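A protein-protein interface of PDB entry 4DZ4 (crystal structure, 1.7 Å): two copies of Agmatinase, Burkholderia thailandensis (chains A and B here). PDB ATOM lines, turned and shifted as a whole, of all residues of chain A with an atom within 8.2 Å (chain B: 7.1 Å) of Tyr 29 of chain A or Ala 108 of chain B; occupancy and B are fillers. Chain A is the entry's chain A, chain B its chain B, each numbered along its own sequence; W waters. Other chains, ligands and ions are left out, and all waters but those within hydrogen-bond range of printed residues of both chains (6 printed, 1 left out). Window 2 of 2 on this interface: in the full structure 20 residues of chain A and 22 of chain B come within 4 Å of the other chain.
OD1 of Asn 27 of chain A touches NE1 of Trp 105 of chain B, 3.6 Å away.
Tyr 29 of chain A touches Pro 55 of chain B.
CD of Arg 67 of chain B touches CG of Tyr 29 of chain A, 3.5 Å away.
Tyr 29 of chain A touches Leu 68 of chain B.
Phe 106 of chain B touches Tyr 29 of chain A (CE1 to OH, 3.9 Å).
Ala 108 of chain B touches Tyr 29 of chain A (CB to OH, 3.5 Å).
Ala 30 of chain A touches Pro 55 of chain B (CB to CG, 3.5 Å).
OD2 of Asp 103 of chain B touches CB of Ala 30 of chain A, at 3.5 Å.
Of chain B, only Pro 55 (3.5 Å), Arg 67 (3.5 Å), Leu 68 (3.5 Å), Phe 106 (3.9 Å) and Ala 108 (3.5 Å) come within 4 Å of Tyr 29 of chain A.
Ala 108 of chain B touches just one residue of chain A: Tyr 29.
Printed residues of chain A within 4 Å of Pro 55 of chain B: Tyr 29 and Ala 30.
Printed residues of chain B within 4 Å of Ala 30 of chain A: Pro 55 (3.5 Å) and Asp 103 (3.5 Å).
Of the printed residues of chain A, Leu 68 of chain B touches Tyr 29.
Val 32 of chain A touches none of the printed residues of chain B.
Ile 114 of chain B touches none of the printed residues of chain A.
The nearest residue of chain B that does not touch Tyr 29 of chain A is Ser 71 of chain B (5.0 Å).
The nearest printed residue of chain A that does not touch Trp 105 of chain B is Glu 26 of chain A (4.4 Å).
No position is printed for both chains.
Of the 10 pairs that touch across the chains among the printed residues, none has its exchanged pair printed and touching as well.
Hydrophobic or aromatic side chains of chain B within 4 Å of the printed part of chain A: Pro 55, Leu 68, Trp 105, Phe 106 and Ala 108.
Of the 12 printed residues of chain A, 4 touch a printed residue of chain B.
Printed residues of chain A that touch a printed residue of chain B: Asn 27, Tyr 29, Ala 30 and Gly 31.
Hydrophobic or aromatic side chains of chain A within 4 Å of the printed part of chain B: Tyr 29 and Ala 30.
Among the printed residues, no Asp or Glu carboxylate lies within 4 Å of a Lys or Arg side-chain nitrogen of the other chain.
ND2 of Asn 27 of chain A lies within hydrogen-bond range of O of Phe 106 of chain B (2.9 Å).
The side-chain carboxylate (OD2) of Asp 103 of chain B sits at hydrogen-bond distance from the backbone NH (N) of Gly 31 of chain A.
Water W1 lies within hydrogen-bond range of OD1 of Asn 27 of chain A, NE1 of Trp 105 of chain B and O of Glu 26 of chain A.
Water W6 lies within hydrogen-bond range of the side-chain amide oxygen of Asn 27 of chain A (2.8 Å), the backbone NH of Ala 108 of chain B (2.9 Å) and the backbone carbonyl oxygen of Phe 106 of chain B (3.1 Å).
Water W3 bridges the side-chain carboxylate of Asp 103 of chain B (2.8 Å) and the backbone NH of Val 32 of chain A (3.4 Å).
Water W5 lies within hydrogen-bond range of OH of Tyr 29 of chain A (2.9 Å), NE2 of His 109 of chain B (3.2 Å) and OD1 of Asn 27 of chain A (3.3 Å).
Water W4 lies within hydrogen-bond range of the side-chain hydroxyl (OH) of Tyr 29 of chain A (2.9 Å) and the guanidinium group (NH2) of Arg 67 of chain B (3.3 Å).
Water W2 lies within hydrogen-bond range of the backbone carbonyl oxygen (O) of Tyr 29 of chain A and the side-chain hydroxyl (OG) of Ser 71 of chain B.
The guanidinium group (NH2) of Arg 37 of chain A sits at hydrogen-bond distance from the backbone carbonyl oxygen (O) of Asn 27 of chain A (3.3 Å).
The guanidinium group (NH1) of Arg 37 of chain A is in hydrogen-bond range of the backbone carbonyl oxygen (O) of Ala 30 of chain A (2.8 Å).
The backbone carbonyl oxygen of Gly 31 of chain A lies within hydrogen-bond range of the guanidinium group of Arg 37 of chain A (3.1 Å).
The side-chain carboxylate (OD1) of Asp 57 of chain B is in salt-bridge range of the guanidinium group (NE) of Arg 67 of chain B (3.0 Å).
OG of Ser 71 of chain B lies within hydrogen-bond range of O of Leu 68 of chain B (2.9 Å).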
ATOM      1  N   GLU A  26     -24.078 -26.047 -36.362  1.00  0.00           N
ATOM      2  CA  GLU A  26     -24.257 -26.983 -35.251  1.00  0.00           C
ATOM      3  C   GLU A  26     -24.721 -26.238 -34.013  1.00  0.00           C
ATOM      4  O   GLU A  26     -24.323 -25.072 -33.806  1.00  0.00           O
ATOM      5  CB  GLU A  26     -22.920 -27.678 -34.898  1.00  0.00           C
ATOM      6  CG  GLU A  26     -22.292 -28.466 -36.050  1.00  0.00           C
ATOM      7  CD  GLU A  26     -22.838 -29.892 -36.161  1.00  0.00           C
ATOM      8  OE1 GLU A  26     -23.801 -30.272 -35.448  1.00  0.00           O
ATOM      9  OE2 GLU A  26     -22.308 -30.642 -36.998  1.00  0.00           O
ATOM     10  N   ASN A  27     -25.540 -26.897 -33.188  1.00  0.00           N
ATOM     11  CA  ASN A  27     -25.646 -26.460 -31.799  1.00  0.00           C
ATOM     12  C   ASN A  27     -24.381 -26.894 -31.085  1.00  0.00           C
ATOM     13  O   ASN A  27     -23.958 -28.043 -31.215  1.00  0.00           O
ATOM     14  CB  ASN A  27     -26.899 -27.026 -31.133  1.00  0.00           C
ATOM     15  CG  ASN A  27     -28.155 -26.264 -31.533  1.00  0.00           C
ATOM     16  OD1 ASN A  27     -28.084 -25.087 -31.923  1.00  0.00           O
ATOM     17  ND2 ASN A  27     -29.307 -26.907 -31.403  1.00  0.00           N
ATOM     18  N   THR A  28     -23.732 -25.949 -30.400  1.00  0.00           N
ATOM     19  CA  THR A  28     -22.385 -26.209 -29.915  1.00  0.00           C
ATOM     20  C   THR A  28     -22.379 -27.350 -28.899  1.00  0.00           C
ATOM     21  O   THR A  28     -21.415 -28.122 -28.828  1.00  0.00           O
ATOM     22  CB  THR A  28     -21.761 -24.942 -29.297  1.00  0.00           C
ATOM     23  OG1 THR A  28     -21.962 -23.842 -30.188  1.00  0.00           O
ATOM     24  CG2 THR A  28     -20.210 -25.151 -29.048  1.00  0.00           C
ATOM     25  N   TYR A  29     -23.477 -27.440 -28.148  1.00  0.00           N
ATOM     26  CA  TYR A  29     -23.695 -28.461 -27.112  1.00  0.00           C
ATOM     27  C   TYR A  29     -24.258 -29.795 -27.620  1.00  0.00           C
ATOM     28  O   TYR A  29     -24.681 -30.619 -26.801  1.00  0.00           O
ATOM     29  CB  TYR A  29     -24.667 -27.879 -26.039  1.00  0.00           C
ATOM     30  CG  TYR A  29     -25.849 -27.142 -26.642  1.00  0.00           C
ATOM     31  CD1 TYR A  29     -27.053 -27.822 -26.943  1.00  0.00           C
ATOM     32  CD2 TYR A  29     -25.775 -25.759 -26.923  1.00  0.00           C
ATOM     33  CE1 TYR A  29     -28.149 -27.122 -27.496  1.00  0.00           C
ATOM     34  CE2 TYR A  29     -26.851 -25.074 -27.473  1.00  0.00           C
ATOM     35  CZ  TYR A  29     -28.028 -25.767 -27.742  1.00  0.00           C
ATOM     36  OH  TYR A  29     -29.085 -25.103 -28.309  1.00  0.00           O
ATOM     37  N   ALA A  30     -24.311 -29.995 -28.947  1.00  0.00           N
ATOM     38  CA  ALA A  30     -24.834 -31.241 -29.483  1.00  0.00           C
ATOM     39  C   ALA A  30     -24.082 -31.588 -30.768  1.00  0.00           C
ATOM     40  O   ALA A  30     -23.046 -30.965 -31.084  1.00  0.00           O
ATOM     41  CB  ALA A  30     -26.330 -31.107 -29.760  1.00  0.00           C
ATOM     42  N   GLY A  31     -24.594 -32.596 -31.486  1.00  0.00           N
ATOM     43  CA  GLY A  31     -24.024 -33.012 -32.764  1.00  0.00           C
ATOM     44  C   GLY A  31     -22.820 -33.934 -32.639  1.00  0.00           C
ATOM     45  O   GLY A  31     -22.141 -33.968 -31.592  1.00  0.00           O
ATOM     46  N   VAL A  32     -22.535 -34.660 -33.720  1.00  0.00           N
ATOM     47  CA  VAL A  32     -21.460 -35.643 -33.734  1.00  0.00           C
ATOM     48  C   VAL A  32     -20.131 -34.998 -33.400  1.00  0.00           C
ATOM     49  O   VAL A  32     -19.801 -33.944 -33.946  1.00  0.00           O
ATOM     50  CB  VAL A  32     -21.400 -36.385 -35.093  1.00  0.00           C
ATOM     51  CG1 VAL A  32     -20.186 -37.309 -35.112  1.00  0.00           C
ATOM     52  CG2 VAL A  32     -22.663 -37.216 -35.265  1.00  0.00           C
ATOM     53  N   LEU A  33     -19.353 -35.636 -32.509  1.00  0.00           N
ATOM     54  CA  LEU A  33     -18.179 -35.010 -31.930  1.00  0.00           C
ATOM     55  C   LEU A  33     -16.874 -35.431 -32.588  1.00  0.00           C
ATOM     56  O   LEU A  33     -15.937 -35.886 -31.914  1.00  0.00           O
ATOM     57  CB  LEU A  33     -18.105 -35.298 -30.419  1.00  0.00           C
ATOM     58  CG  LEU A  33     -19.302 -34.722 -29.618  1.00  0.00           C
ATOM     59  CD1 LEU A  33     -19.258 -35.299 -28.200  1.00  0.00           C
ATOM     60  CD2 LEU A  33     -19.257 -33.195 -29.567  1.00  0.00           C
ATOM     61  N   ARG A  37     -15.712 -30.976 -35.962  1.00  0.00           N
ATOM     62  CA  ARG A  37     -16.866 -31.419 -36.752  1.00  0.00           C
ATOM     63  C   ARG A  37     -16.497 -31.907 -38.141  1.00  0.00           C
ATOM     64  O   ARG A  37     -17.372 -31.983 -38.993  1.00  0.00           O
ATOM     65  CB  ARG A  37     -17.938 -30.311 -36.913  1.00  0.00           C
ATOM     66  CG  ARG A  37     -18.301 -29.534 -35.643  1.00  0.00           C
ATOM     67  CD  ARG A  37     -18.945 -30.458 -34.626  1.00  0.00           C
ATOM     68  NE  ARG A  37     -19.559 -29.636 -33.593  1.00  0.00           N
ATOM     69  CZ  ARG A  37     -20.423 -30.094 -32.684  1.00  0.00           C
ATOM     70  NH1 ARG A  37     -20.746 -31.381 -32.635  1.00  0.00           N
ATOM     71  NH2 ARG A  37     -20.959 -29.242 -31.825  1.00  0.00           N
ATOM     72  N   ALA A  75     -14.082 -33.519 -28.071  1.00  0.00           N
ATOM     73  CA  ALA A  75     -15.192 -32.860 -27.375  1.00  0.00           C
ATOM     74  C   ALA A  75     -14.868 -31.364 -27.128  1.00  0.00           C
ATOM     75  O   ALA A  75     -15.783 -30.509 -27.194  1.00  0.00           O
ATOM     76  CB  ALA A  75     -15.483 -33.545 -26.052  1.00  0.00           C
ATOM     77  N   VAL A  78     -15.471 -28.214 -29.949  1.00  0.00           N
ATOM     78  CA  VAL A  78     -16.780 -27.738 -30.445  1.00  0.00           C
ATOM     79  C   VAL A  78     -16.898 -26.220 -30.671  1.00  0.00           C
ATOM     80  O   VAL A  78     -17.437 -25.770 -31.681  1.00  0.00           O
ATOM     81  CB  VAL A  78     -17.958 -28.337 -29.643  1.00  0.00           C
ATOM     82  CG1 VAL A  78     -18.030 -29.868 -29.843  1.00  0.00           C
ATOM     83  CG2 VAL A  78     -17.888 -27.989 -28.144  1.00  0.00           C
ATOM     84  N   GLN A  79     -16.367 -25.402 -29.768  1.00  0.00           N
ATOM     85  CA  GLN A  79     -16.471 -23.944 -29.986  1.00  0.00           C
ATOM     86  C   GLN A  79     -15.598 -23.495 -31.153  1.00  0.00           C
ATOM     87  O   GLN A  79     -15.964 -22.559 -31.859  1.00  0.00           O
ATOM     88  CB  GLN A  79     -16.007 -23.199 -28.760  1.00  0.00           C
ATOM     89  CG  GLN A  79     -16.928 -23.373 -27.588  1.00  0.00           C
ATOM     90  CD  GLN A  79     -16.376 -22.628 -26.412  1.00  0.00           C
ATOM     91  OE1 GLN A  79     -16.581 -21.412 -26.285  1.00  0.00           O
ATOM     92  NE2 GLN A  79     -15.620 -23.336 -25.575  1.00  0.00           N
ATOM     93  N   PRO B  55     -31.276 -32.227 -27.384  1.00  0.00           N
ATOM     94  CA  PRO B  55     -30.388 -31.612 -26.365  1.00  0.00           C
ATOM     95  C   PRO B  55     -30.984 -30.322 -25.795  1.00  0.00           C
ATOM     96  O   PRO B  55     -30.425 -29.229 -25.953  1.00  0.00           O
ATOM     97  CB  PRO B  55     -29.120 -31.307 -27.166  1.00  0.00           C
ATOM     98  CG  PRO B  55     -29.643 -31.005 -28.544  1.00  0.00           C
ATOM     99  CD  PRO B  55     -30.744 -32.035 -28.754  1.00  0.00           C
ATOM    100  N   LEU B  56     -32.110 -30.471 -25.117  1.00  0.00           N
ATOM    101  CA  LEU B  56     -32.866 -29.319 -24.595  1.00  0.00           C
ATOM    102  C   LEU B  56     -32.687 -29.179 -23.093  1.00  0.00           C
ATOM    103  O   LEU B  56     -32.810 -30.172 -22.358  1.00  0.00           O
ATOM    104  CB  LEU B  56     -34.344 -29.551 -24.868  1.00  0.00           C
ATOM    105  CG  LEU B  56     -35.324 -28.475 -24.396  1.00  0.00           C
ATOM    106  CD1 LEU B  56     -35.130 -27.147 -25.160  1.00  0.00           C
ATOM    107  CD2 LEU B  56     -36.781 -28.943 -24.526  1.00  0.00           C
ATOM    108  N   ASP B  57     -32.448 -27.969 -22.593  1.00  0.00           N
ATOM    109  CA  ASP B  57     -32.635 -27.756 -21.143  1.00  0.00           C
ATOM    110  C   ASP B  57     -33.301 -26.414 -20.832  1.00  0.00           C
ATOM    111  O   ASP B  57     -33.309 -25.951 -19.691  1.00  0.00           O
ATOM    112  CB  ASP B  57     -31.350 -27.974 -20.298  1.00  0.00           C
ATOM    113  CG  ASP B  57     -30.226 -27.017 -20.663  1.00  0.00           C
ATOM    114  OD1 ASP B  57     -30.479 -26.056 -21.388  1.00  0.00           O
ATOM    115  OD2 ASP B  57     -29.089 -27.275 -20.214  1.00  0.00           O
ATOM    116  N   LEU B  58     -33.915 -25.823 -21.849  1.00  0.00           N
ATOM    117  CA  LEU B  58     -34.603 -24.530 -21.670  1.00  0.00           C
ATOM    118  C   LEU B  58     -35.862 -24.616 -20.814  1.00  0.00           C
ATOM    119  O   LEU B  58     -36.352 -23.609 -20.314  1.00  0.00           O
ATOM    120  CB  LEU B  58     -34.940 -23.896 -23.045  1.00  0.00           C
ATOM    121  CG  LEU B  58     -33.736 -23.729 -23.973  1.00  0.00           C
ATOM    122  CD1 LEU B  58     -34.170 -23.184 -25.329  1.00  0.00           C
ATOM    123  CD2 LEU B  58     -32.686 -22.798 -23.350  1.00  0.00           C
ATOM    124  N   ARG B  67     -28.949 -30.243 -21.517  1.00  0.00           N
ATOM    125  CA  ARG B  67     -28.663 -30.117 -22.952  1.00  0.00           C
ATOM    126  C   ARG B  67     -27.500 -31.028 -23.406  1.00  0.00           C
ATOM    127  O   ARG B  67     -27.440 -31.425 -24.557  1.00  0.00           O
ATOM    128  CB  ARG B  67     -28.398 -28.645 -23.342  1.00  0.00           C
ATOM    129  CG  ARG B  67     -27.106 -28.072 -22.768  1.00  0.00           C
ATOM    130  CD  ARG B  67     -26.840 -26.646 -23.326  1.00  0.00           C
ATOM    131  NE  ARG B  67     -27.904 -25.736 -22.881  1.00  0.00           N
ATOM    132  CZ  ARG B  67     -27.982 -24.450 -23.176  1.00  0.00           C
ATOM    133  NH1 ARG B  67     -27.017 -23.856 -23.885  1.00  0.00           N
ATOM    134  NH2 ARG B  67     -29.027 -23.748 -22.739  1.00  0.00           N
ATOM    135  N   LEU B  68     -26.569 -31.325 -22.501  1.00  0.00           N
ATOM    136  CA  LEU B  68     -25.449 -32.177 -22.811  1.00  0.00           C
ATOM    137  C   LEU B  68     -25.727 -33.666 -22.520  1.00  0.00           C
ATOM    138  O   LEU B  68     -24.859 -34.522 -22.684  1.00  0.00           O
ATOM    139  CB  LEU B  68     -24.237 -31.686 -22.021  1.00  0.00           C
ATOM    140  CG  LEU B  68     -23.612 -30.361 -22.489  1.00  0.00           C
ATOM    141  CD1 LEU B  68     -22.650 -29.900 -21.395  1.00  0.00           C
ATOM    142  CD2 LEU B  68     -22.895 -30.528 -23.823  1.00  0.00           C
ATOM    143  N   GLY B  69     -26.935 -33.963 -22.074  1.00  0.00           N
ATOM    144  CA  GLY B  69     -27.298 -35.346 -21.722  1.00  0.00           C
ATOM    145  C   GLY B  69     -27.058 -36.378 -22.835  1.00  0.00           C
ATOM    146  O   GLY B  69     -26.531 -37.457 -22.573  1.00  0.00           O
ATOM    147  N   PRO B  70     -27.443 -36.067 -24.077  1.00  0.00           N
ATOM    148  CA  PRO B  70     -27.285 -37.119 -25.086  1.00  0.00           C
ATOM    149  C   PRO B  70     -25.836 -37.523 -25.299  1.00  0.00           C
ATOM    150  O   PRO B  70     -25.534 -38.720 -25.405  1.00  0.00           O
ATOM    151  CB  PRO B  70     -27.879 -36.474 -26.353  1.00  0.00           C
ATOM    152  CG  PRO B  70     -28.939 -35.559 -25.802  1.00  0.00           C
ATOM    153  CD  PRO B  70     -28.280 -34.959 -24.572  1.00  0.00           C
ATOM    154  N   SER B  71     -24.930 -36.536 -25.336  1.00  0.00           N
ATOM    155  CA  SER B  71     -23.508 -36.855 -25.502  1.00  0.00           C
ATOM    156  C   SER B  71     -23.006 -37.664 -24.314  1.00  0.00           C
ATOM    157  O   SER B  71     -22.163 -38.541 -24.470  1.00  0.00           O
ATOM    158  CB  SER B  71     -22.662 -35.572 -25.716  1.00  0.00           C
ATOM    159  OG  SER B  71     -22.747 -34.700 -24.609  1.00  0.00           O
ATOM    160  N   ASP B 103     -28.655 -36.001 -33.576  1.00  0.00           N
ATOM    161  CA  ASP B 103     -29.570 -35.207 -32.753  1.00  0.00           C
ATOM    162  C   ASP B 103     -30.614 -34.407 -33.524  1.00  0.00           C
ATOM    163  O   ASP B 103     -30.444 -34.090 -34.710  1.00  0.00           O
ATOM    164  CB  ASP B 103     -28.759 -34.222 -31.887  1.00  0.00           C
ATOM    165  CG  ASP B 103     -27.826 -34.923 -30.914  1.00  0.00           C
ATOM    166  OD1 ASP B 103     -28.201 -35.984 -30.347  1.00  0.00           O
ATOM    167  OD2 ASP B 103     -26.692 -34.432 -30.713  1.00  0.00           O
ATOM    168  N   TRP B 105     -31.823 -31.112 -34.350  1.00  0.00           N
ATOM    169  CA  TRP B 105     -31.432 -29.710 -34.366  1.00  0.00           C
ATOM    170  C   TRP B 105     -32.605 -28.808 -34.060  1.00  0.00           C
ATOM    171  O   TRP B 105     -33.753 -29.068 -34.461  1.00  0.00           O
ATOM    172  CB  TRP B 105     -30.792 -29.332 -35.713  1.00  0.00           C
ATOM    173  CG  TRP B 105     -30.272 -27.916 -35.682  1.00  0.00           C
ATOM    174  CD1 TRP B 105     -29.029 -27.472 -35.203  1.00  0.00           C
ATOM    175  CD2 TRP B 105     -31.003 -26.709 -36.054  1.00  0.00           C
ATOM    176  NE1 TRP B 105     -28.935 -26.101 -35.297  1.00  0.00           N
ATOM    177  CE2 TRP B 105     -30.101 -25.576 -35.779  1.00  0.00           C
ATOM    178  CE3 TRP B 105     -32.276 -26.458 -36.565  1.00  0.00           C
ATOM    179  CZ2 TRP B 105     -30.476 -24.254 -36.043  1.00  0.00           C
ATOM    180  CZ3 TRP B 105     -32.645 -25.128 -36.811  1.00  0.00           C
ATOM    181  CH2 TRP B 105     -31.762 -24.054 -36.558  1.00  0.00           C
ATOM    182  N   PHE B 106     -32.350 -27.740 -33.310  1.00  0.00           N
ATOM    183  CA  PHE B 106     -33.367 -26.701 -33.135  1.00  0.00           C
ATOM    184  C   PHE B 106     -32.675 -25.369 -32.886  1.00  0.00           C
ATOM    185  O   PHE B 106     -31.506 -25.329 -32.500  1.00  0.00           O
ATOM    186  CB  PHE B 106     -34.365 -27.025 -32.016  1.00  0.00           C
ATOM    187  CG  PHE B 106     -33.717 -27.250 -30.674  1.00  0.00           C
ATOM    188  CD1 PHE B 106     -33.374 -26.162 -29.880  1.00  0.00           C
ATOM    189  CD2 PHE B 106     -33.464 -28.534 -30.212  1.00  0.00           C
ATOM    190  CE1 PHE B 106     -32.760 -26.361 -28.640  1.00  0.00           C
ATOM    191  CE2 PHE B 106     -32.867 -28.742 -28.987  1.00  0.00           C
ATOM    192  CZ  PHE B 106     -32.490 -27.656 -28.205  1.00  0.00           C
ATOM    193  N   ASP B 107     -33.419 -24.296 -33.121  1.00  0.00           N
ATOM    194  CA  ASP B 107     -32.925 -22.944 -32.939  1.00  0.00           C
ATOM    195  C   ASP B 107     -33.366 -22.469 -31.552  1.00  0.00           C
ATOM    196  O   ASP B 107     -34.503 -22.010 -31.371  1.00  0.00           O
ATOM    197  CB  ASP B 107     -33.531 -22.075 -34.034  1.00  0.00           C
ATOM    198  CG  ASP B 107     -33.086 -20.636 -33.953  1.00  0.00           C
ATOM    199  OD1 ASP B 107     -32.266 -20.299 -33.071  1.00  0.00           O
ATOM    200  OD2 ASP B 107     -33.587 -19.851 -34.795  1.00  0.00           O
ATOM    201  N   ALA B 108     -32.467 -22.633 -30.570  1.00  0.00           N
ATOM    202  CA  ALA B 108     -32.735 -22.279 -29.182  1.00  0.00           C
ATOM    203  C   ALA B 108     -33.107 -20.821 -29.026  1.00  0.00           C
ATOM    204  O   ALA B 108     -33.805 -20.450 -28.077  1.00  0.00           O
ATOM    205  CB  ALA B 108     -31.507 -22.578 -28.313  1.00  0.00           C
ATOM    206  N   HIS B 109     -32.664 -19.984 -29.956  1.00  0.00           N
ATOM    207  CA  HIS B 109     -32.843 -18.547 -29.839  1.00  0.00           C
ATOM    208  C   HIS B 109     -34.204 -18.104 -30.308  1.00  0.00           C
ATOM    209  O   HIS B 109     -34.568 -16.941 -30.121  1.00  0.00           O
ATOM    210  CB  HIS B 109     -31.640 -17.801 -30.461  1.00  0.00           C
ATOM    211  CG  HIS B 109     -30.319 -18.446 -30.082  1.00  0.00           C
ATOM    212  ND1 HIS B 109     -29.836 -18.426 -28.810  1.00  0.00           N
ATOM    213  CD2 HIS B 109     -29.441 -19.256 -30.821  1.00  0.00           C
ATOM    214  CE1 HIS B 109     -28.696 -19.158 -28.740  1.00  0.00           C
ATOM    215  NE2 HIS B 109     -28.447 -19.660 -29.974  1.00  0.00           N
ATOM    216  N   HIS B 110     -34.965 -19.056 -30.885  1.00  0.00           N
ATOM    217  CA  HIS B 110     -36.420 -18.924 -31.151  1.00  0.00           C
ATOM    218  C   HIS B 110     -37.185 -20.033 -30.485  1.00  0.00           C
ATOM    219  O   HIS B 110     -37.622 -20.999 -31.111  1.00  0.00           O
ATOM    220  CB  HIS B 110     -36.717 -18.857 -32.640  1.00  0.00           C
ATOM    221  CG  HIS B 110     -36.185 -17.609 -33.273  1.00  0.00           C
ATOM    222  ND1 HIS B 110     -34.984 -17.567 -33.878  1.00  0.00           N
ATOM    223  CD2 HIS B 110     -36.694 -16.306 -33.302  1.00  0.00           C
ATOM    224  CE1 HIS B 110     -34.744 -16.309 -34.322  1.00  0.00           C
ATOM    225  NE2 HIS B 110     -35.794 -15.535 -33.962  1.00  0.00           N
ATOM    226  N   PRO B 111     -37.343 -19.924 -29.173  1.00  0.00           N
ATOM    227  CA  PRO B 111     -37.820 -21.068 -28.387  1.00  0.00           C
ATOM    228  C   PRO B 111     -39.223 -21.594 -28.737  1.00  0.00           C
ATOM    229  O   PRO B 111     -39.504 -22.788 -28.498  1.00  0.00           O
ATOM    230  CB  PRO B 111     -37.775 -20.571 -26.939  1.00  0.00           C
ATOM    231  CG  PRO B 111     -37.406 -19.139 -26.985  1.00  0.00           C
ATOM    232  CD  PRO B 111     -37.036 -18.730 -28.367  1.00  0.00           C
ATOM    233  N   LEU B 112     -40.070 -20.764 -29.331  1.00  0.00           N
ATOM    234  CA  LEU B 112     -41.388 -21.272 -29.741  1.00  0.00           C
ATOM    235  C   LEU B 112     -41.297 -22.238 -30.939  1.00  0.00           C
ATOM    236  O   LEU B 112     -42.271 -22.951 -31.237  1.00  0.00           O
ATOM    237  CB  LEU B 112     -42.382 -20.147 -30.013  1.00  0.00           C
ATOM    238  CG  LEU B 112     -42.704 -19.206 -28.830  1.00  0.00           C
ATOM    239  CD1 LEU B 112     -43.690 -18.136 -29.223  1.00  0.00           C
ATOM    240  CD2 LEU B 112     -43.166 -19.963 -27.592  1.00  0.00           C
ATOM    241  N   SER B 113     -40.155 -22.256 -31.632  1.00  0.00           N
ATOM    242  CA  SER B 113     -39.917 -23.219 -32.734  1.00  0.00           C
ATOM    243  C   SER B 113     -39.493 -24.614 -32.252  1.00  0.00           C
ATOM    244  O   SER B 113     -39.410 -25.546 -33.059  1.00  0.00           O
ATOM    245  CB  SER B 113     -38.856 -22.671 -33.706  1.00  0.00           C
ATOM    246  OG  SER B 113     -37.546 -22.782 -33.128  1.00  0.00           O
ATOM    247  N   ILE B 114     -39.206 -24.762 -30.954  1.00  0.00           N
ATOM    248  CA  ILE B 114     -38.620 -26.013 -30.442  1.00  0.00           C
ATOM    249  C   ILE B 114     -39.621 -27.166 -30.436  1.00  0.00           C
ATOM    250  O   ILE B 114     -39.325 -28.264 -30.937  1.00  0.00           O
ATOM    251  CB  ILE B 114     -37.957 -25.794 -29.066  1.00  0.00           C
ATOM    252  CG1 ILE B 114     -36.764 -24.822 -29.245  1.00  0.00           C
ATOM    253  CG2 ILE B 114     -37.495 -27.122 -28.445  1.00  0.00           C
ATOM    254  CD1 ILE B 114     -36.198 -24.358 -27.914  1.00  0.00           C
ATOM    255  N   LEU B 177     -42.754 -23.557 -21.741  1.00  0.00           N
ATOM    256  CA  LEU B 177     -41.700 -24.513 -21.982  1.00  0.00           C
ATOM    257  C   LEU B 177     -41.278 -24.904 -20.587  1.00  0.00           C
ATOM    258  O   LEU B 177     -40.475 -24.198 -19.986  1.00  0.00           O
ATOM    259  CB  LEU B 177     -40.570 -23.783 -22.710  1.00  0.00           C
ATOM    260  CG  LEU B 177     -39.394 -24.483 -23.375  1.00  0.00           C
ATOM    261  CD1 LEU B 177     -39.849 -25.728 -24.126  1.00  0.00           C
ATOM    262  CD2 LEU B 177     -38.781 -23.492 -24.369  1.00  0.00           C
HETATM  263  O   HOH W   1     -27.237 -23.838 -34.184  1.00  0.00           O
HETATM  264  O   HOH W   2     -22.263 -32.496 -26.983  1.00  0.00           O
HETATM  265  O   HOH W   3     -25.431 -36.130 -32.617  1.00  0.00           O
HETATM  266  O   HOH W   4     -30.292 -24.289 -25.781  1.00  0.00           O
HETATM  267  O   HOH W   5     -27.965 -22.752 -29.559  1.00  0.00           O
HETATM  268  O   HOH W   6     -29.816 -22.873 -31.602  1.00  0.00           O
